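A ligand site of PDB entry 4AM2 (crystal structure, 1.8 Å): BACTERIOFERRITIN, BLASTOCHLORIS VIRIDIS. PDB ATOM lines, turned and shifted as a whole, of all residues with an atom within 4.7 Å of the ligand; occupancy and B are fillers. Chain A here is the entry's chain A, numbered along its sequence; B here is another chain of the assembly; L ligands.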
ATOM      1  N   LEU A  19     -34.862  -3.637  17.102  1.00  0.00           N
ATOM      2  CA  LEU A  19     -34.169  -2.386  17.210  1.00  0.00           C
ATOM      3  C   LEU A  19     -34.766  -1.477  18.308  1.00  0.00           C
ATOM      4  O   LEU A  19     -34.057  -0.698  18.928  1.00  0.00           O
ATOM      5  CB  LEU A  19     -34.345  -1.565  15.896  1.00  0.00           C
ATOM      6  CG  LEU A  19     -33.627  -2.187  14.684  1.00  0.00           C
ATOM      7  CD1 LEU A  19     -34.126  -1.492  13.409  1.00  0.00           C
ATOM      8  CD2 LEU A  19     -32.119  -2.098  14.866  1.00  0.00           C
ATOM      9  N   VAL A  22     -33.408  -2.876  21.528  1.00  0.00           N
ATOM     10  CA  VAL A  22     -32.010  -2.558  21.741  1.00  0.00           C
ATOM     11  C   VAL A  22     -31.885  -1.135  22.400  1.00  0.00           C
ATOM     12  O   VAL A  22     -31.080  -0.951  23.384  1.00  0.00           O
ATOM     13  CB  VAL A  22     -31.244  -2.470  20.373  1.00  0.00           C
ATOM     14  CG1 VAL A  22     -29.844  -1.814  20.552  1.00  0.00           C
ATOM     15  CG2 VAL A  22     -31.032  -3.879  19.887  1.00  0.00           C
ATOM     16  N   SER A  23     -32.514  -0.145  21.788  1.00  0.00           N
ATOM     17  CA  SER A  23     -32.447   1.245  22.276  1.00  0.00           C
ATOM     18  C   SER A  23     -33.109   1.455  23.608  1.00  0.00           C
ATOM     19  O   SER A  23     -32.602   2.226  24.470  1.00  0.00           O
ATOM     20  CB  SER A  23     -33.017   2.260  21.275  1.00  0.00           C
ATOM     21  OG  SER A  23     -32.126   2.367  20.195  1.00  0.00           O
ATOM     22  N   TRP A  26     -30.860  -0.129  26.143  1.00  0.00           N
ATOM     23  CA  TRP A  26     -29.576   0.602  26.311  1.00  0.00           C
ATOM     24  C   TRP A  26     -29.872   1.875  27.087  1.00  0.00           C
ATOM     25  O   TRP A  26     -29.105   2.313  27.975  1.00  0.00           O
ATOM     26  CB  TRP A  26     -28.988   1.029  24.924  1.00  0.00           C
ATOM     27  CG  TRP A  26     -27.546   1.442  25.124  1.00  0.00           C
ATOM     28  CD1 TRP A  26     -27.051   2.705  25.412  1.00  0.00           C
ATOM     29  CD2 TRP A  26     -26.414   0.525  25.262  1.00  0.00           C
ATOM     30  NE1 TRP A  26     -25.719   2.636  25.706  1.00  0.00           N
ATOM     31  CE2 TRP A  26     -25.258   1.371  25.569  1.00  0.00           C
ATOM     32  CE3 TRP A  26     -26.248  -0.841  25.119  1.00  0.00           C
ATOM     33  CZ2 TRP A  26     -23.995   0.826  25.767  1.00  0.00           C
ATOM     34  CZ3 TRP A  26     -24.968  -1.377  25.269  1.00  0.00           C
ATOM     35  CH2 TRP A  26     -23.872  -0.567  25.595  1.00  0.00           C
ATOM     36  N   ARG A  45     -27.412  -3.651  30.248  1.00  0.00           N
ATOM     37  CA  ARG A  45     -26.408  -3.560  29.114  1.00  0.00           C
ATOM     38  C   ARG A  45     -26.322  -4.919  28.432  1.00  0.00           C
ATOM     39  O   ARG A  45     -26.300  -5.011  27.143  1.00  0.00           O
ATOM     40  CB  ARG A  45     -25.054  -3.159  29.729  1.00  0.00           C
ATOM     41  CG  ARG A  45     -24.042  -2.808  28.654  1.00  0.00           C
ATOM     42  CD  ARG A  45     -22.689  -2.577  29.296  1.00  0.00           C
ATOM     43  NE  ARG A  45     -21.754  -1.861  28.391  1.00  0.00           N
ATOM     44  CZ  ARG A  45     -20.953  -2.441  27.558  1.00  0.00           C
ATOM     45  NH1 ARG A  45     -20.971  -3.735  27.468  1.00  0.00           N
ATOM     46  NH2 ARG A  45     -20.099  -1.703  26.833  1.00  0.00           N
ATOM     47  N   ILE A  49     -27.430  -5.973  24.487  1.00  0.00           N
ATOM     48  CA  ILE A  49     -26.460  -6.601  23.524  1.00  0.00           C
ATOM     49  C   ILE A  49     -27.033  -7.958  23.016  1.00  0.00           C
ATOM     50  O   ILE A  49     -26.820  -8.328  21.828  1.00  0.00           O
ATOM     51  CB  ILE A  49     -25.076  -6.754  24.216  1.00  0.00           C
ATOM     52  CG1 ILE A  49     -24.474  -5.352  24.330  1.00  0.00           C
ATOM     53  CG2 ILE A  49     -24.077  -7.630  23.420  1.00  0.00           C
ATOM     54  CD1 ILE A  49     -23.235  -5.205  25.269  1.00  0.00           C
ATOM     55  N   MET A  52     -29.218  -6.926  20.335  1.00  0.00           N
ATOM     56  CA  MET A  52     -28.485  -6.537  19.143  1.00  0.00           C
ATOM     57  C   MET A  52     -28.267  -7.753  18.235  1.00  0.00           C
ATOM     58  O   MET A  52     -28.364  -7.627  17.020  1.00  0.00           O
ATOM     59  CB  MET A  52     -27.139  -5.852  19.429  1.00  0.00           C
ATOM     60  CG  MET A  52     -27.397  -4.479  20.173  1.00  0.00           C
ATOM     61  SD  MET A  52     -25.781  -3.912  20.807  1.00  0.00           S
ATOM     62  CE  MET A  52     -26.386  -2.805  22.114  1.00  0.00           C
ATOM     63  N   ALA A  53     -27.907  -8.868  18.822  1.00  0.00           N
ATOM     64  CA  ALA A  53     -27.669 -10.089  18.096  1.00  0.00           C
ATOM     65  C   ALA A  53     -28.943 -10.600  17.415  1.00  0.00           C
ATOM     66  O   ALA A  53     -28.875 -11.106  16.304  1.00  0.00           O
ATOM     67  CB  ALA A  53     -27.005 -11.116  19.028  1.00  0.00           C
ATOM     68  N   ALA A  55     -31.360  -8.601  16.347  1.00  0.00           N
ATOM     69  CA  ALA A  55     -31.624  -7.636  15.216  1.00  0.00           C
ATOM     70  C   ALA A  55     -30.766  -8.124  14.040  1.00  0.00           C
ATOM     71  O   ALA A  55     -31.254  -8.187  12.918  1.00  0.00           O
ATOM     72  CB  ALA A  55     -31.256  -6.215  15.603  1.00  0.00           C
ATOM     73  N   ASP A  56     -29.520  -8.473  14.337  1.00  0.00           N
ATOM     74  CA  ASP A  56     -28.621  -8.865  13.284  1.00  0.00           C
ATOM     75  C   ASP A  56     -29.130 -10.176  12.614  1.00  0.00           C
ATOM     76  O   ASP A  56     -29.124 -10.282  11.403  1.00  0.00           O
ATOM     77  CB  ASP A  56     -27.235  -9.078  13.897  1.00  0.00           C
ATOM     78  CG  ASP A  56     -26.205  -9.479  12.841  1.00  0.00           C
ATOM     79  OD1 ASP A  56     -26.175  -8.952  11.742  1.00  0.00           O
ATOM     80  OD2 ASP A  56     -25.419 -10.387  13.074  1.00  0.00           O
ATOM     81  N   LEU A  71     -34.203  -0.556   8.626  1.00  0.00           N
ATOM     82  CA  LEU A  71     -33.763  -0.146   9.991  1.00  0.00           C
ATOM     83  C   LEU A  71     -34.177   1.318  10.252  1.00  0.00           C
ATOM     84  O   LEU A  71     -33.744   1.911  11.252  1.00  0.00           O
ATOM     85  CB  LEU A  71     -32.235  -0.314  10.139  1.00  0.00           C
ATOM     86  CG  LEU A  71     -31.763  -1.767  10.098  1.00  0.00           C
ATOM     87  CD1 LEU A  71     -31.748  -2.282   8.656  1.00  0.00           C
ATOM     88  CD2 LEU A  71     -30.370  -1.849  10.756  1.00  0.00           C
ATOM     89  N   LEU B  19     -26.859   7.167  15.923  1.00  0.00           N
ATOM     90  CA  LEU B  19     -27.794   6.022  15.723  1.00  0.00           C
ATOM     91  C   LEU B  19     -28.017   5.709  14.244  1.00  0.00           C
ATOM     92  O   LEU B  19     -28.182   4.579  13.850  1.00  0.00           O
ATOM     93  CB  LEU B  19     -29.186   6.299  16.362  1.00  0.00           C
ATOM     94  CG  LEU B  19     -29.064   6.355  17.914  1.00  0.00           C
ATOM     95  CD1 LEU B  19     -30.360   6.985  18.495  1.00  0.00           C
ATOM     96  CD2 LEU B  19     -28.721   5.020  18.527  1.00  0.00           C
ATOM     97  N   VAL B  22     -24.843   3.997  13.104  1.00  0.00           N
ATOM     98  CA  VAL B  22     -24.788   2.623  13.520  1.00  0.00           C
ATOM     99  C   VAL B  22     -25.601   1.721  12.520  1.00  0.00           C
ATOM    100  O   VAL B  22     -25.075   0.695  12.049  1.00  0.00           O
ATOM    101  CB  VAL B  22     -25.369   2.422  14.953  1.00  0.00           C
ATOM    102  CG1 VAL B  22     -25.552   0.916  15.264  1.00  0.00           C
ATOM    103  CG2 VAL B  22     -24.395   3.018  15.976  1.00  0.00           C
ATOM    104  N   SER B  23     -26.869   2.038  12.286  1.00  0.00           N
ATOM    105  CA  SER B  23     -27.717   1.247  11.462  1.00  0.00           C
ATOM    106  C   SER B  23     -27.323   1.226   9.997  1.00  0.00           C
ATOM    107  O   SER B  23     -27.438   0.155   9.330  1.00  0.00           O
ATOM    108  CB  SER B  23     -29.166   1.729  11.570  1.00  0.00           C
ATOM    109  OG  SER B  23     -29.685   1.261  12.796  1.00  0.00           O
ATOM    110  N   TRP B  26     -24.294  -0.900   9.769  1.00  0.00           N
ATOM    111  CA  TRP B  26     -24.538  -2.327  10.051  1.00  0.00           C
ATOM    112  C   TRP B  26     -25.252  -2.908   8.814  1.00  0.00           C
ATOM    113  O   TRP B  26     -25.012  -4.059   8.380  1.00  0.00           O
ATOM    114  CB  TRP B  26     -25.491  -2.510  11.257  1.00  0.00           C
ATOM    115  CG  TRP B  26     -25.436  -3.959  11.700  1.00  0.00           C
ATOM    116  CD1 TRP B  26     -26.269  -4.992  11.295  1.00  0.00           C
ATOM    117  CD2 TRP B  26     -24.395  -4.569  12.494  1.00  0.00           C
ATOM    118  NE1 TRP B  26     -25.829  -6.185  11.828  1.00  0.00           N
ATOM    119  CE2 TRP B  26     -24.732  -5.993  12.596  1.00  0.00           C
ATOM    120  CE3 TRP B  26     -23.278  -4.071  13.200  1.00  0.00           C
ATOM    121  CZ2 TRP B  26     -23.926  -6.887  13.329  1.00  0.00           C
ATOM    122  CZ3 TRP B  26     -22.512  -4.943  13.954  1.00  0.00           C
ATOM    123  CH2 TRP B  26     -22.797  -6.330  13.997  1.00  0.00           C
ATOM    124  N   ARG B  45     -18.535  -3.722   9.655  1.00  0.00           N
ATOM    125  CA  ARG B  45     -19.018  -4.203  10.965  1.00  0.00           C
ATOM    126  C   ARG B  45     -18.215  -3.455  12.078  1.00  0.00           C
ATOM    127  O   ARG B  45     -18.794  -2.959  13.087  1.00  0.00           O
ATOM    128  CB  ARG B  45     -18.795  -5.712  11.052  1.00  0.00           C
ATOM    129  CG  ARG B  45     -19.264  -6.303  12.406  1.00  0.00           C
ATOM    130  CD  ARG B  45     -19.054  -7.802  12.412  1.00  0.00           C
ATOM    131  NE  ARG B  45     -19.957  -8.536  13.300  1.00  0.00           N
ATOM    132  CZ  ARG B  45     -19.769  -8.682  14.589  1.00  0.00           C
ATOM    133  NH1 ARG B  45     -18.724  -8.136  15.136  1.00  0.00           N
ATOM    134  NH2 ARG B  45     -20.586  -9.419  15.313  1.00  0.00           N
ATOM    135  N   ILE B  49     -19.681  -0.769  14.962  1.00  0.00           N
ATOM    136  CA  ILE B  49     -19.372  -0.874  16.416  1.00  0.00           C
ATOM    137  C   ILE B  49     -18.651   0.368  16.990  1.00  0.00           C
ATOM    138  O   ILE B  49     -18.917   0.779  18.131  1.00  0.00           O
ATOM    139  CB  ILE B  49     -18.610  -2.223  16.674  1.00  0.00           C
ATOM    140  CG1 ILE B  49     -19.615  -3.357  16.378  1.00  0.00           C
ATOM    141  CG2 ILE B  49     -18.198  -2.349  18.153  1.00  0.00           C
ATOM    142  CD1 ILE B  49     -18.944  -4.762  16.378  1.00  0.00           C
ATOM    143  N   MET B  52     -21.336   2.722  17.568  1.00  0.00           N
ATOM    144  CA  MET B  52     -22.137   2.367  18.739  1.00  0.00           C
ATOM    145  C   MET B  52     -21.489   2.976  19.986  1.00  0.00           C
ATOM    146  O   MET B  52     -22.213   3.454  20.857  1.00  0.00           O
ATOM    147  CB  MET B  52     -22.267   0.858  18.942  1.00  0.00           C
ATOM    148  CG  MET B  52     -23.158   0.211  17.840  1.00  0.00           C
ATOM    149  SD  MET B  52     -22.936  -1.618  17.921  1.00  0.00           S
ATOM    150  CE  MET B  52     -23.314  -1.972  16.188  1.00  0.00           C
ATOM    151  N   ALA B  55     -22.444   6.616  20.062  1.00  0.00           N
ATOM    152  CA  ALA B  55     -23.834   6.803  20.512  1.00  0.00           C
ATOM    153  C   ALA B  55     -23.905   6.719  22.054  1.00  0.00           C
ATOM    154  O   ALA B  55     -24.529   7.588  22.690  1.00  0.00           O
ATOM    155  CB  ALA B  55     -24.793   5.768  19.869  1.00  0.00           C
ATOM    156  N   ASP B  56     -23.269   5.697  22.618  1.00  0.00           N
ATOM    157  CA  ASP B  56     -23.225   5.537  24.028  1.00  0.00           C
ATOM    158  C   ASP B  56     -22.650   6.798  24.757  1.00  0.00           C
ATOM    159  O   ASP B  56     -23.180   7.197  25.814  1.00  0.00           O
ATOM    160  CB  ASP B  56     -22.443   4.276  24.401  1.00  0.00           C
ATOM    161  CG  ASP B  56     -22.491   4.008  25.890  1.00  0.00           C
ATOM    162  OD1 ASP B  56     -23.522   4.172  26.569  1.00  0.00           O
ATOM    163  OD2 ASP B  56     -21.408   3.731  26.446  1.00  0.00           O
HETATM  164  C1  LIG L   1     -21.755  -4.477  20.398  1.00  0.00           C
HETATM  165  C2  LIG L   1     -25.046  -4.994  16.845  1.00  0.00           C
HETATM  166  C3  LIG L   1     -27.178  -0.819  18.086  1.00  0.00           C
HETATM  167  C4  LIG L   1     -23.761  -0.263  21.645  1.00  0.00           C
HETATM  168  C5  LIG L   1     -22.594  -5.043  19.408  1.00  0.00           C
HETATM  169  C6  LIG L   1     -22.439  -6.422  18.951  1.00  0.00           C
HETATM  170  C7  LIG L   1     -23.381  -6.610  17.855  1.00  0.00           C
HETATM  171  C8  LIG L   1     -24.053  -5.294  17.824  1.00  0.00           C
HETATM  172  C9  LIG L   1     -23.771  -7.857  17.059  1.00  0.00           C
HETATM  173  C10 LIG L   1     -21.490  -7.353  19.658  1.00  0.00           C
HETATM  174  C11 LIG L   1     -20.304  -7.256  18.745  1.00  0.00           C
HETATM  175  C12 LIG L   1     -19.456  -8.477  19.132  1.00  0.00           C
HETATM  176  O1  LIG L   1     -18.627  -8.840  18.247  1.00  0.00           O
HETATM  177  O2  LIG L   1     -19.669  -9.016  20.276  1.00  0.00           O
HETATM  178  C13 LIG L   1     -25.936  -3.861  16.874  1.00  0.00           C
HETATM  179  C14 LIG L   1     -26.987  -3.681  15.837  1.00  0.00           C
HETATM  180  C15 LIG L   1     -27.493  -2.417  16.222  1.00  0.00           C
HETATM  181  C16 LIG L   1     -26.795  -1.999  17.427  1.00  0.00           C
HETATM  182  C17 LIG L   1     -27.394  -4.543  14.641  1.00  0.00           C
HETATM  183  C18 LIG L   1     -28.650  -1.659  15.700  1.00  0.00           C
HETATM  184  C19 LIG L   1     -28.344  -1.456  14.435  1.00  0.00           C
HETATM  185  C20 LIG L   1     -26.497  -0.387  19.268  1.00  0.00           C
HETATM  186  C21 LIG L   1     -26.893   0.846  19.940  1.00  0.00           C
HETATM  187  C22 LIG L   1     -25.861   1.021  20.912  1.00  0.00           C
HETATM  188  C23 LIG L   1     -24.926  -0.119  20.833  1.00  0.00           C
HETATM  189  C24 LIG L   1     -28.145   1.674  19.642  1.00  0.00           C
HETATM  190  C25 LIG L   1     -25.796   2.050  22.026  1.00  0.00           C
HETATM  191  C26 LIG L   1     -26.458   3.167  21.862  1.00  0.00           C
HETATM  192  C27 LIG L   1     -22.872  -1.424  21.573  1.00  0.00           C
HETATM  193  C28 LIG L   1     -21.717  -1.422  22.408  1.00  0.00           C
HETATM  194  C29 LIG L   1     -21.103  -2.689  22.064  1.00  0.00           C
HETATM  195  C30 LIG L   1     -21.969  -3.207  21.023  1.00  0.00           C
HETATM  196  C31 LIG L   1     -21.362  -0.293  23.329  1.00  0.00           C
HETATM  197  C32 LIG L   1     -19.841  -3.341  22.557  1.00  0.00           C
HETATM  198  C33 LIG L   1     -20.241  -3.924  23.892  1.00  0.00           C
HETATM  199  C34 LIG L   1     -18.939  -4.377  24.545  1.00  0.00           C
HETATM  200  O3  LIG L   1     -17.884  -4.431  23.820  1.00  0.00           O
HETATM  201  O4  LIG L   1     -19.007  -4.673  25.763  1.00  0.00           O
HETATM  202  N1  LIG L   1     -23.538  -4.275  18.663  1.00  0.00           N
HETATM  203  N2  LIG L   1     -25.809  -2.841  17.808  1.00  0.00           N
HETATM  204  N3  LIG L   1     -25.223  -0.905  19.695  1.00  0.00           N
HETATM  205  N4  LIG L   1     -23.032  -2.424  20.724  1.00  0.00           N
HETATM  206 FE1  LIG L   1     -24.520  -2.647  19.293  1.00  0.00          FE
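Residues that only touch the ligand: Leu 19 of chain A (3.6 Å), Val 22 of chain A (3.8 Å), Trp 26 of chain A (3.4 Å), Ile 49 of chain A (3.5 Å), Leu 19 of chain B (3.6 Å), Val 22 of chain B (3.7 Å), Ser 23 of chain B (3.4 Å), Trp 26 of chain B (3.6 Å), Ile 49 of chain B (3.7 Å) and Ala 55 of chain B (3.7 Å). Hydrophobic or aromatic side chains that line the ligand: Leu 19 of chain A, Val 22 of chain A, Trp 26 of chain A, Ile 49 of chain A, Met 52 of chain A, Leu 19 of chain B, Val 22 of chain B, Trp 26 of chain B, Ile 49 of chain B, Met 52 of chain B and Ala 55 of chain B. Of the 20 residues printed, 14 come within 4 Å of the ligand. Along chain A the residues within 4 Å of the ligand span positions 19 to 52.
The side-chain carboxylate (OD1) of Asp 56 of chain B is in hydrogen-bond range of the indole nitrogen (NE1) of Trp 26 of chain A, 2.8 Å away. The indole nitrogen (NE1) of Trp 26 of chain B lies within hydrogen-bond range of the side-chain carboxylate (OD1) of Asp 56 of chain A.
The side-chain sulfur of Met 52 of chain A binds an iron atom (FE1) of the ligand, 2.3 Å away. An oxygen (O1) of the ligand lies within salt-bridge range of the guanidinium group of Arg 45 of chain B, 3.2 Å away. NH1 of Arg 45 of chain A lies within salt-bridge range of O4 of the ligand. SD of Met 52 of chain B is bound to FE1 of the ligand, at 2.3 Å.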
